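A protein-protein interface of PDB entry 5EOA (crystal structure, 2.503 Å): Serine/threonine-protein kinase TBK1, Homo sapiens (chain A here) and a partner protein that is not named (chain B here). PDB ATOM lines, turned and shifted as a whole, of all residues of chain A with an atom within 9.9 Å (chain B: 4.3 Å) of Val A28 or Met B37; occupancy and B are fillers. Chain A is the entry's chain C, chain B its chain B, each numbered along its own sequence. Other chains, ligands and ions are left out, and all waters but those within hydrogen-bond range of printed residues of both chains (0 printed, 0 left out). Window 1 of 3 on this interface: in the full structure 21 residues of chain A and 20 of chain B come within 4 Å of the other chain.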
ATOM      1  N   LYS A  20      -0.074   2.633  28.944  1.00  0.00           N
ATOM      2  CA  LYS A  20       0.480   3.415  27.856  1.00  0.00           C
ATOM      3  C   LYS A  20      -0.607   4.250  27.214  1.00  0.00           C
ATOM      4  O   LYS A  20      -0.403   5.426  26.933  1.00  0.00           O
ATOM      5  CB  LYS A  20       1.081   2.488  26.813  1.00  0.00           C
ATOM      6  CG  LYS A  20       2.381   2.987  26.212  1.00  0.00           C
ATOM      7  CD  LYS A  20       2.255   4.363  25.578  1.00  0.00           C
ATOM      8  CE  LYS A  20       3.618   4.881  25.178  1.00  0.00           C
ATOM      9  NZ  LYS A  20       4.356   3.871  24.372  1.00  0.00           N
ATOM     10  N   LEU A  21      -1.757   3.634  26.971  1.00  0.00           N
ATOM     11  CA  LEU A  21      -2.881   4.340  26.371  1.00  0.00           C
ATOM     12  C   LEU A  21      -3.318   5.487  27.272  1.00  0.00           C
ATOM     13  O   LEU A  21      -3.626   6.575  26.794  1.00  0.00           O
ATOM     14  CB  LEU A  21      -4.042   3.373  26.151  1.00  0.00           C
ATOM     15  CG  LEU A  21      -4.483   3.085  24.712  1.00  0.00           C
ATOM     16  CD1 LEU A  21      -3.337   3.175  23.741  1.00  0.00           C
ATOM     17  CD2 LEU A  21      -5.117   1.714  24.637  1.00  0.00           C
ATOM     18  N   LYS A  22      -3.320   5.230  28.578  1.00  0.00           N
ATOM     19  CA  LYS A  22      -3.730   6.212  29.567  1.00  0.00           C
ATOM     20  C   LYS A  22      -2.780   7.409  29.539  1.00  0.00           C
ATOM     21  O   LYS A  22      -3.198   8.576  29.545  1.00  0.00           O
ATOM     22  CB  LYS A  22      -3.718   5.554  30.947  1.00  0.00           C
ATOM     23  CG  LYS A  22      -4.955   5.815  31.777  1.00  0.00           C
ATOM     24  CD  LYS A  22      -4.801   7.070  32.617  1.00  0.00           C
ATOM     25  CE  LYS A  22      -4.046   6.780  33.898  1.00  0.00           C
ATOM     26  NZ  LYS A  22      -4.860   5.931  34.808  1.00  0.00           N
ATOM     27  N   GLU A  23      -1.495   7.090  29.488  1.00  0.00           N
ATOM     28  CA  GLU A  23      -0.426   8.070  29.448  1.00  0.00           C
ATOM     29  C   GLU A  23      -0.474   8.838  28.144  1.00  0.00           C
ATOM     30  O   GLU A  23      -0.348  10.054  28.132  1.00  0.00           O
ATOM     31  CB  GLU A  23       0.912   7.340  29.582  1.00  0.00           C
ATOM     32  CG  GLU A  23       2.160   8.195  29.463  1.00  0.00           C
ATOM     33  CD  GLU A  23       3.431   7.359  29.591  1.00  0.00           C
ATOM     34  OE1 GLU A  23       3.320   6.120  29.752  1.00  0.00           O
ATOM     35  OE2 GLU A  23       4.540   7.935  29.530  1.00  0.00           O
ATOM     36  N   GLU A  24      -0.664   8.125  27.042  1.00  0.00           N
ATOM     37  CA  GLU A  24      -0.698   8.764  25.740  1.00  0.00           C
ATOM     38  C   GLU A  24      -1.883   9.722  25.684  1.00  0.00           C
ATOM     39  O   GLU A  24      -1.786  10.815  25.124  1.00  0.00           O
ATOM     40  CB  GLU A  24      -0.787   7.716  24.632  1.00  0.00           C
ATOM     41  CG  GLU A  24      -0.090   8.110  23.332  1.00  0.00           C
ATOM     42  CD  GLU A  24       1.325   7.560  23.229  1.00  0.00           C
ATOM     43  OE1 GLU A  24       1.757   7.214  22.108  1.00  0.00           O
ATOM     44  OE2 GLU A  24       2.013   7.482  24.267  1.00  0.00           O
ATOM     45  N   MET A  25      -2.990   9.326  26.303  1.00  0.00           N
ATOM     46  CA  MET A  25      -4.173  10.164  26.333  1.00  0.00           C
ATOM     47  C   MET A  25      -3.974  11.444  27.152  1.00  0.00           C
ATOM     48  O   MET A  25      -4.488  12.502  26.798  1.00  0.00           O
ATOM     49  CB  MET A  25      -5.369   9.369  26.837  1.00  0.00           C
ATOM     50  CG  MET A  25      -6.056   8.616  25.716  1.00  0.00           C
ATOM     51  SD  MET A  25      -6.656   9.763  24.446  1.00  0.00           S
ATOM     52  CE  MET A  25      -7.722  10.788  25.467  1.00  0.00           C
ATOM     53  N   GLU A  26      -3.207  11.343  28.227  1.00  0.00           N
ATOM     54  CA  GLU A  26      -2.870  12.495  29.034  1.00  0.00           C
ATOM     55  C   GLU A  26      -2.152  13.562  28.192  1.00  0.00           C
ATOM     56  O   GLU A  26      -2.365  14.767  28.382  1.00  0.00           O
ATOM     57  CB  GLU A  26      -2.020  12.059  30.233  1.00  0.00           C
ATOM     58  CG  GLU A  26      -2.815  11.264  31.274  1.00  0.00           C
ATOM     59  CD  GLU A  26      -1.934  10.529  32.281  1.00  0.00           C
ATOM     60  OE1 GLU A  26      -0.690  10.553  32.125  1.00  0.00           O
ATOM     61  OE2 GLU A  26      -2.493   9.922  33.228  1.00  0.00           O
ATOM     62  N   GLY A  27      -1.315  13.121  27.256  1.00  0.00           N
ATOM     63  CA  GLY A  27      -0.591  14.041  26.394  1.00  0.00           C
ATOM     64  C   GLY A  27      -1.486  14.599  25.306  1.00  0.00           C
ATOM     65  O   GLY A  27      -1.330  15.739  24.867  1.00  0.00           O
ATOM     66  N   VAL A  28      -2.437  13.785  24.869  1.00  0.00           N
ATOM     67  CA  VAL A  28      -3.392  14.223  23.875  1.00  0.00           C
ATOM     68  C   VAL A  28      -4.295  15.333  24.425  1.00  0.00           C
ATOM     69  O   VAL A  28      -4.512  16.339  23.752  1.00  0.00           O
ATOM     70  CB  VAL A  28      -4.204  13.038  23.354  1.00  0.00           C
ATOM     71  CG1 VAL A  28      -5.393  13.505  22.545  1.00  0.00           C
ATOM     72  CG2 VAL A  28      -3.300  12.138  22.520  1.00  0.00           C
ATOM     73  N   VAL A  29      -4.801  15.171  25.645  1.00  0.00           N
ATOM     74  CA  VAL A  29      -5.635  16.217  26.221  1.00  0.00           C
ATOM     75  C   VAL A  29      -4.822  17.492  26.460  1.00  0.00           C
ATOM     76  O   VAL A  29      -5.340  18.608  26.328  1.00  0.00           O
ATOM     77  CB  VAL A  29      -6.367  15.758  27.500  1.00  0.00           C
ATOM     78  CG1 VAL A  29      -7.226  14.572  27.182  1.00  0.00           C
ATOM     79  CG2 VAL A  29      -5.389  15.399  28.574  1.00  0.00           C
ATOM     80  N   LYS A  30      -3.549  17.317  26.796  1.00  0.00           N
ATOM     81  CA  LYS A  30      -2.608  18.424  26.856  1.00  0.00           C
ATOM     82  C   LYS A  30      -2.628  19.243  25.546  1.00  0.00           C
ATOM     83  O   LYS A  30      -2.782  20.465  25.576  1.00  0.00           O
ATOM     84  CB  LYS A  30      -1.202  17.886  27.127  1.00  0.00           C
ATOM     85  CG  LYS A  30      -0.544  18.391  28.397  1.00  0.00           C
ATOM     86  CD  LYS A  30      -1.243  17.872  29.639  1.00  0.00           C
ATOM     87  CE  LYS A  30      -0.399  18.118  30.877  1.00  0.00           C
ATOM     88  NZ  LYS A  30       0.926  17.445  30.787  1.00  0.00           N
ATOM     89  N   GLU A  31      -2.486  18.560  24.408  1.00  0.00           N
ATOM     90  CA  GLU A  31      -2.511  19.204  23.100  1.00  0.00           C
ATOM     91  C   GLU A  31      -3.855  19.882  22.877  1.00  0.00           C
ATOM     92  O   GLU A  31      -3.937  20.986  22.329  1.00  0.00           O
ATOM     93  CB  GLU A  31      -2.310  18.173  21.979  1.00  0.00           C
ATOM     94  CG  GLU A  31      -0.972  17.462  21.980  1.00  0.00           C
ATOM     95  CD  GLU A  31       0.197  18.385  21.711  1.00  0.00           C
ATOM     96  OE1 GLU A  31       0.072  19.276  20.860  1.00  0.00           O
ATOM     97  OE2 GLU A  31       1.252  18.216  22.347  1.00  0.00           O
ATOM     98  N   LEU A  32      -4.912  19.199  23.288  1.00  0.00           N
ATOM     99  CA  LEU A  32      -6.244  19.731  23.131  1.00  0.00           C
ATOM    100  C   LEU A  32      -6.304  21.070  23.852  1.00  0.00           C
ATOM    101  O   LEU A  32      -6.804  22.042  23.305  1.00  0.00           O
ATOM    102  CB  LEU A  32      -7.259  18.755  23.707  1.00  0.00           C
ATOM    103  CG  LEU A  32      -8.709  18.911  23.260  1.00  0.00           C
ATOM    104  CD1 LEU A  32      -9.555  19.370  24.444  1.00  0.00           C
ATOM    105  CD2 LEU A  32      -8.822  19.857  22.054  1.00  0.00           C
ATOM    106  N   ALA A  33      -5.749  21.111  25.060  1.00  0.00           N
ATOM    107  CA  ALA A  33      -5.721  22.325  25.867  1.00  0.00           C
ATOM    108  C   ALA A  33      -4.982  23.483  25.185  1.00  0.00           C
ATOM    109  O   ALA A  33      -5.420  24.639  25.265  1.00  0.00           O
ATOM    110  CB  ALA A  33      -5.106  22.031  27.223  1.00  0.00           C
ATOM    111  N   GLU A  34      -3.863  23.173  24.532  1.00  0.00           N
ATOM    112  CA  GLU A  34      -3.086  24.176  23.810  1.00  0.00           C
ATOM    113  C   GLU A  34      -3.913  24.739  22.644  1.00  0.00           C
ATOM    114  O   GLU A  34      -4.079  25.958  22.508  1.00  0.00           O
ATOM    115  CB  GLU A  34      -1.770  23.568  23.312  1.00  0.00           C
ATOM    116  CG  GLU A  34      -0.820  24.558  22.656  1.00  0.00           C
ATOM    117  CD  GLU A  34      -0.344  25.637  23.611  1.00  0.00           C
ATOM    118  OE1 GLU A  34      -0.265  25.360  24.830  1.00  0.00           O
ATOM    119  OE2 GLU A  34      -0.049  26.765  23.145  1.00  0.00           O
ATOM    120  N   ASN A  35      -4.430  23.833  21.820  1.00  0.00           N
ATOM    121  CA  ASN A  35      -5.390  24.161  20.777  1.00  0.00           C
ATOM    122  C   ASN A  35      -6.483  25.122  21.266  1.00  0.00           C
ATOM    123  O   ASN A  35      -6.719  26.159  20.660  1.00  0.00           O
ATOM    124  CB  ASN A  35      -6.014  22.864  20.259  1.00  0.00           C
ATOM    125  CG  ASN A  35      -6.484  22.972  18.835  1.00  0.00           C
ATOM    126  OD1 ASN A  35      -7.685  23.100  18.568  1.00  0.00           O
ATOM    127  ND2 ASN A  35      -5.541  22.903  17.900  1.00  0.00           N
ATOM    128  N   ASN A  36      -7.131  24.785  22.376  1.00  0.00           N
ATOM    129  CA  ASN A  36      -8.139  25.659  22.971  1.00  0.00           C
ATOM    130  C   ASN A  36      -7.569  27.039  23.325  1.00  0.00           C
ATOM    131  O   ASN A  36      -8.236  28.051  23.173  1.00  0.00           O
ATOM    132  CB  ASN A  36      -8.746  25.036  24.239  1.00  0.00           C
ATOM    133  CG  ASN A  36      -9.623  23.824  23.951  1.00  0.00           C
ATOM    134  OD1 ASN A  36     -10.258  23.726  22.901  1.00  0.00           O
ATOM    135  ND2 ASN A  36      -9.672  22.898  24.904  1.00  0.00           N
ATOM    136  N   ILE A  38      -5.129  28.763  21.974  1.00  0.00           N
ATOM    137  CA  ILE A  38      -4.915  29.529  20.765  1.00  0.00           C
ATOM    138  C   ILE A  38      -6.250  29.941  20.146  1.00  0.00           C
ATOM    139  O   ILE A  38      -6.427  31.089  19.753  1.00  0.00           O
ATOM    140  CB  ILE A  38      -4.054  28.720  19.783  1.00  0.00           C
ATOM    141  CG1 ILE A  38      -2.691  28.453  20.413  1.00  0.00           C
ATOM    142  CG2 ILE A  38      -3.879  29.442  18.468  1.00  0.00           C
ATOM    143  CD1 ILE A  38      -1.931  27.342  19.760  1.00  0.00           C
ATOM    144  N   LEU B  33      -2.318   9.737  16.565  1.00  0.00           N
ATOM    145  CA  LEU B  33      -3.137  10.866  16.948  1.00  0.00           C
ATOM    146  C   LEU B  33      -2.347  11.913  17.728  1.00  0.00           C
ATOM    147  O   LEU B  33      -2.562  13.113  17.558  1.00  0.00           O
ATOM    148  CB  LEU B  33      -4.304  10.387  17.795  1.00  0.00           C
ATOM    149  CG  LEU B  33      -5.176  11.502  18.346  1.00  0.00           C
ATOM    150  CD1 LEU B  33      -6.039  12.080  17.225  1.00  0.00           C
ATOM    151  CD2 LEU B  33      -6.014  11.028  19.520  1.00  0.00           C
ATOM    152  N   LYS B  34      -1.433  11.461  18.580  1.00  0.00           N
ATOM    153  CA  LYS B  34      -0.644  12.390  19.375  1.00  0.00           C
ATOM    154  C   LYS B  34       0.209  13.243  18.456  1.00  0.00           C
ATOM    155  O   LYS B  34       0.147  14.468  18.504  1.00  0.00           O
ATOM    156  CB  LYS B  34       0.230  11.653  20.397  1.00  0.00           C
ATOM    157  CG  LYS B  34       0.839  12.574  21.458  1.00  0.00           C
ATOM    158  CD  LYS B  34       1.685  11.799  22.460  1.00  0.00           C
ATOM    159  CE  LYS B  34       2.744  10.953  21.765  1.00  0.00           C
ATOM    160  NZ  LYS B  34       3.434  10.000  22.696  1.00  0.00           N
ATOM    161  N   GLU B  35       0.979  12.588  17.597  1.00  0.00           N
ATOM    162  CA  GLU B  35       1.844  13.289  16.662  1.00  0.00           C
ATOM    163  C   GLU B  35       1.048  14.173  15.710  1.00  0.00           C
ATOM    164  O   GLU B  35       1.483  15.265  15.358  1.00  0.00           O
ATOM    165  CB  GLU B  35       2.698  12.296  15.873  1.00  0.00           C
ATOM    166  CG  GLU B  35       3.785  11.646  16.705  1.00  0.00           C
ATOM    167  CD  GLU B  35       4.594  12.658  17.501  1.00  0.00           C
ATOM    168  OE1 GLU B  35       5.172  13.587  16.885  1.00  0.00           O
ATOM    169  OE2 GLU B  35       4.640  12.528  18.747  1.00  0.00           O
ATOM    170  N   ALA B  36      -0.117  13.688  15.301  1.00  0.00           N
ATOM    171  CA  ALA B  36      -0.983  14.427  14.420  1.00  0.00           C
ATOM    172  C   ALA B  36      -1.416  15.709  15.124  1.00  0.00           C
ATOM    173  O   ALA B  36      -1.350  16.804  14.551  1.00  0.00           O
ATOM    174  CB  ALA B  36      -2.178  13.590  14.052  1.00  0.00           C
ATOM    175  N   MET B  37      -1.839  15.574  16.376  1.00  0.00           N
ATOM    176  CA  MET B  37      -2.283  16.725  17.140  1.00  0.00           C
ATOM    177  C   MET B  37      -1.157  17.739  17.379  1.00  0.00           C
ATOM    178  O   MET B  37      -1.383  18.940  17.301  1.00  0.00           O
ATOM    179  CB  MET B  37      -2.901  16.279  18.455  1.00  0.00           C
ATOM    180  CG  MET B  37      -4.334  15.795  18.322  1.00  0.00           C
ATOM    181  SD  MET B  37      -5.271  16.340  19.740  1.00  0.00           S
ATOM    182  CE  MET B  37      -5.025  18.124  19.603  1.00  0.00           C
ATOM    183  N   LYS B  38       0.043  17.243  17.667  1.00  0.00           N
ATOM    184  CA  LYS B  38       1.228  18.083  17.776  1.00  0.00           C
ATOM    185  C   LYS B  38       1.409  18.915  16.511  1.00  0.00           C
ATOM    186  O   LYS B  38       1.730  20.107  16.578  1.00  0.00           O
ATOM    187  CB  LYS B  38       2.468  17.216  17.978  1.00  0.00           C
ATOM    188  CG  LYS B  38       3.317  17.587  19.170  1.00  0.00           C
ATOM    189  CD  LYS B  38       3.039  16.667  20.346  1.00  0.00           C
ATOM    190  CE  LYS B  38       3.717  15.316  20.174  1.00  0.00           C
ATOM    191  NZ  LYS B  38       5.205  15.414  20.218  1.00  0.00           N
ATOM    192  N   LEU B  39       1.201  18.283  15.360  1.00  0.00           N
ATOM    193  CA  LEU B  39       1.329  18.955  14.067  1.00  0.00           C
ATOM    194  C   LEU B  39       0.181  19.931  13.894  1.00  0.00           C
ATOM    195  O   LEU B  39       0.334  21.006  13.310  1.00  0.00           O
ATOM    196  CB  LEU B  39       1.299  17.940  12.926  1.00  0.00           C
ATOM    197  CG  LEU B  39       2.553  17.758  12.068  1.00  0.00           C
ATOM    198  CD1 LEU B  39       3.677  18.641  12.551  1.00  0.00           C
ATOM    199  CD2 LEU B  39       2.997  16.291  12.042  1.00  0.00           C
ATOM    200  N   ASN B  40      -0.982  19.543  14.401  1.00  0.00           N
ATOM    201  CA  ASN B  40      -2.130  20.413  14.325  1.00  0.00           C
ATOM    202  C   ASN B  40      -1.894  21.680  15.137  1.00  0.00           C
ATOM    203  O   ASN B  40      -2.141  22.787  14.656  1.00  0.00           O
ATOM    204  CB  ASN B  40      -3.365  19.697  14.823  1.00  0.00           C
ATOM    205  CG  ASN B  40      -4.531  20.623  14.964  1.00  0.00           C
ATOM    206  OD1 ASN B  40      -4.780  21.148  16.047  1.00  0.00           O
ATOM    207  ND2 ASN B  40      -5.252  20.849  13.867  1.00  0.00           N
ATOM    208  N   ASN B  41      -1.401  21.517  16.363  1.00  0.00           N
ATOM    209  CA  ASN B  41      -1.110  22.660  17.211  1.00  0.00           C
ATOM    210  C   ASN B  41      -0.042  23.584  16.660  1.00  0.00           C
ATOM    211  O   ASN B  41      -0.164  24.786  16.799  1.00  0.00           O
ATOM    212  CB  ASN B  41      -0.780  22.226  18.632  1.00  0.00           C
ATOM    213  CG  ASN B  41      -2.019  22.018  19.456  1.00  0.00           C
ATOM    214  OD1 ASN B  41      -3.043  22.678  19.243  1.00  0.00           O
ATOM    215  ND2 ASN B  41      -1.949  21.091  20.395  1.00  0.00           N
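Printed residues of chain B within 4 Å of Val A28: Leu B33 (3.96 Å) and Met B37 (3.99 Å). Printed residues of chain A within 4 Å of Met B37: Val A28 (3.99 Å), Glu A31 (3.6 Å) and Leu A32 (3.8 Å). No residue of chain A comes within 4 Å of Ala B36. Of chain A, only Asn A35 comes within 4 Å of Asn B40. Of the printed residues of chain B, Leu A32 touches Met B37. Of the printed residues of chain A, Leu B33 touches Val A28 (3.96 Å). Lys A20 touches none of the printed residues of chain B. The nearest printed residue of chain B that does not touch Val A28 is Lys B34 (4.1 Å). The nearest printed residue of chain B that does not touch Glu A34 is Met B37 (7.2 Å).
Among the printed residues, merely in contact across the chains: Val A28 with Leu B33 (3.96 Å), Val A28 with Met B37 (3.99 Å), Glu A31 with Met B37 (3.6 Å), Glu A31 with Lys B38 (3.1 Å), Leu A32 with Met B37 (3.8 Å) and Glu A34 with Asn B41 (3.8 Å).
Printed residues of chain B that touch a printed residue of chain A: Leu B33, Lys B34, Met B37, Lys B38, Asn B40 and Asn B41. Hydrophobic or aromatic side chains of chain B that line the printed part of chain A: Leu B33 and Met B37. Printed residues of chain A that touch a printed residue of chain B: Glu A24, Val A28, Glu A31, Leu A32, Glu A34 and Asn A35. Among the printed residues, Asp or Glu carboxylates within 4 Å of a Lys or Arg side-chain nitrogen of the other chain: Glu A24 with Lys B34.
The side-chain amino group (NZ) of Lys B38 is in salt-bridge range of the side-chain carboxylate (OE2) of Glu B35 (3.3 Å). ND2 of Asn A36 sits at hydrogen-bond distance from O of Leu A32 (3.4 Å).
The side-chain carboxylate (OE2) of Glu A24 is in salt-bridge range of the side-chain amino group (NZ) of Lys B34, at 3.3 Å. The side-chain amide oxygen of Asn B40 lies within hydrogen-bond range of the side-chain amide nitrogen of Asn A35 (2.7 Å). The side-chain amide nitrogen (ND2) of Asn B41 lies within hydrogen-bond range of the side-chain carboxylate (OE1) of Glu A31, 2.8 Å away. OD1 of Asn B41 sits at hydrogen-bond distance from ND2 of Asn A35, 2.8 Å away.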
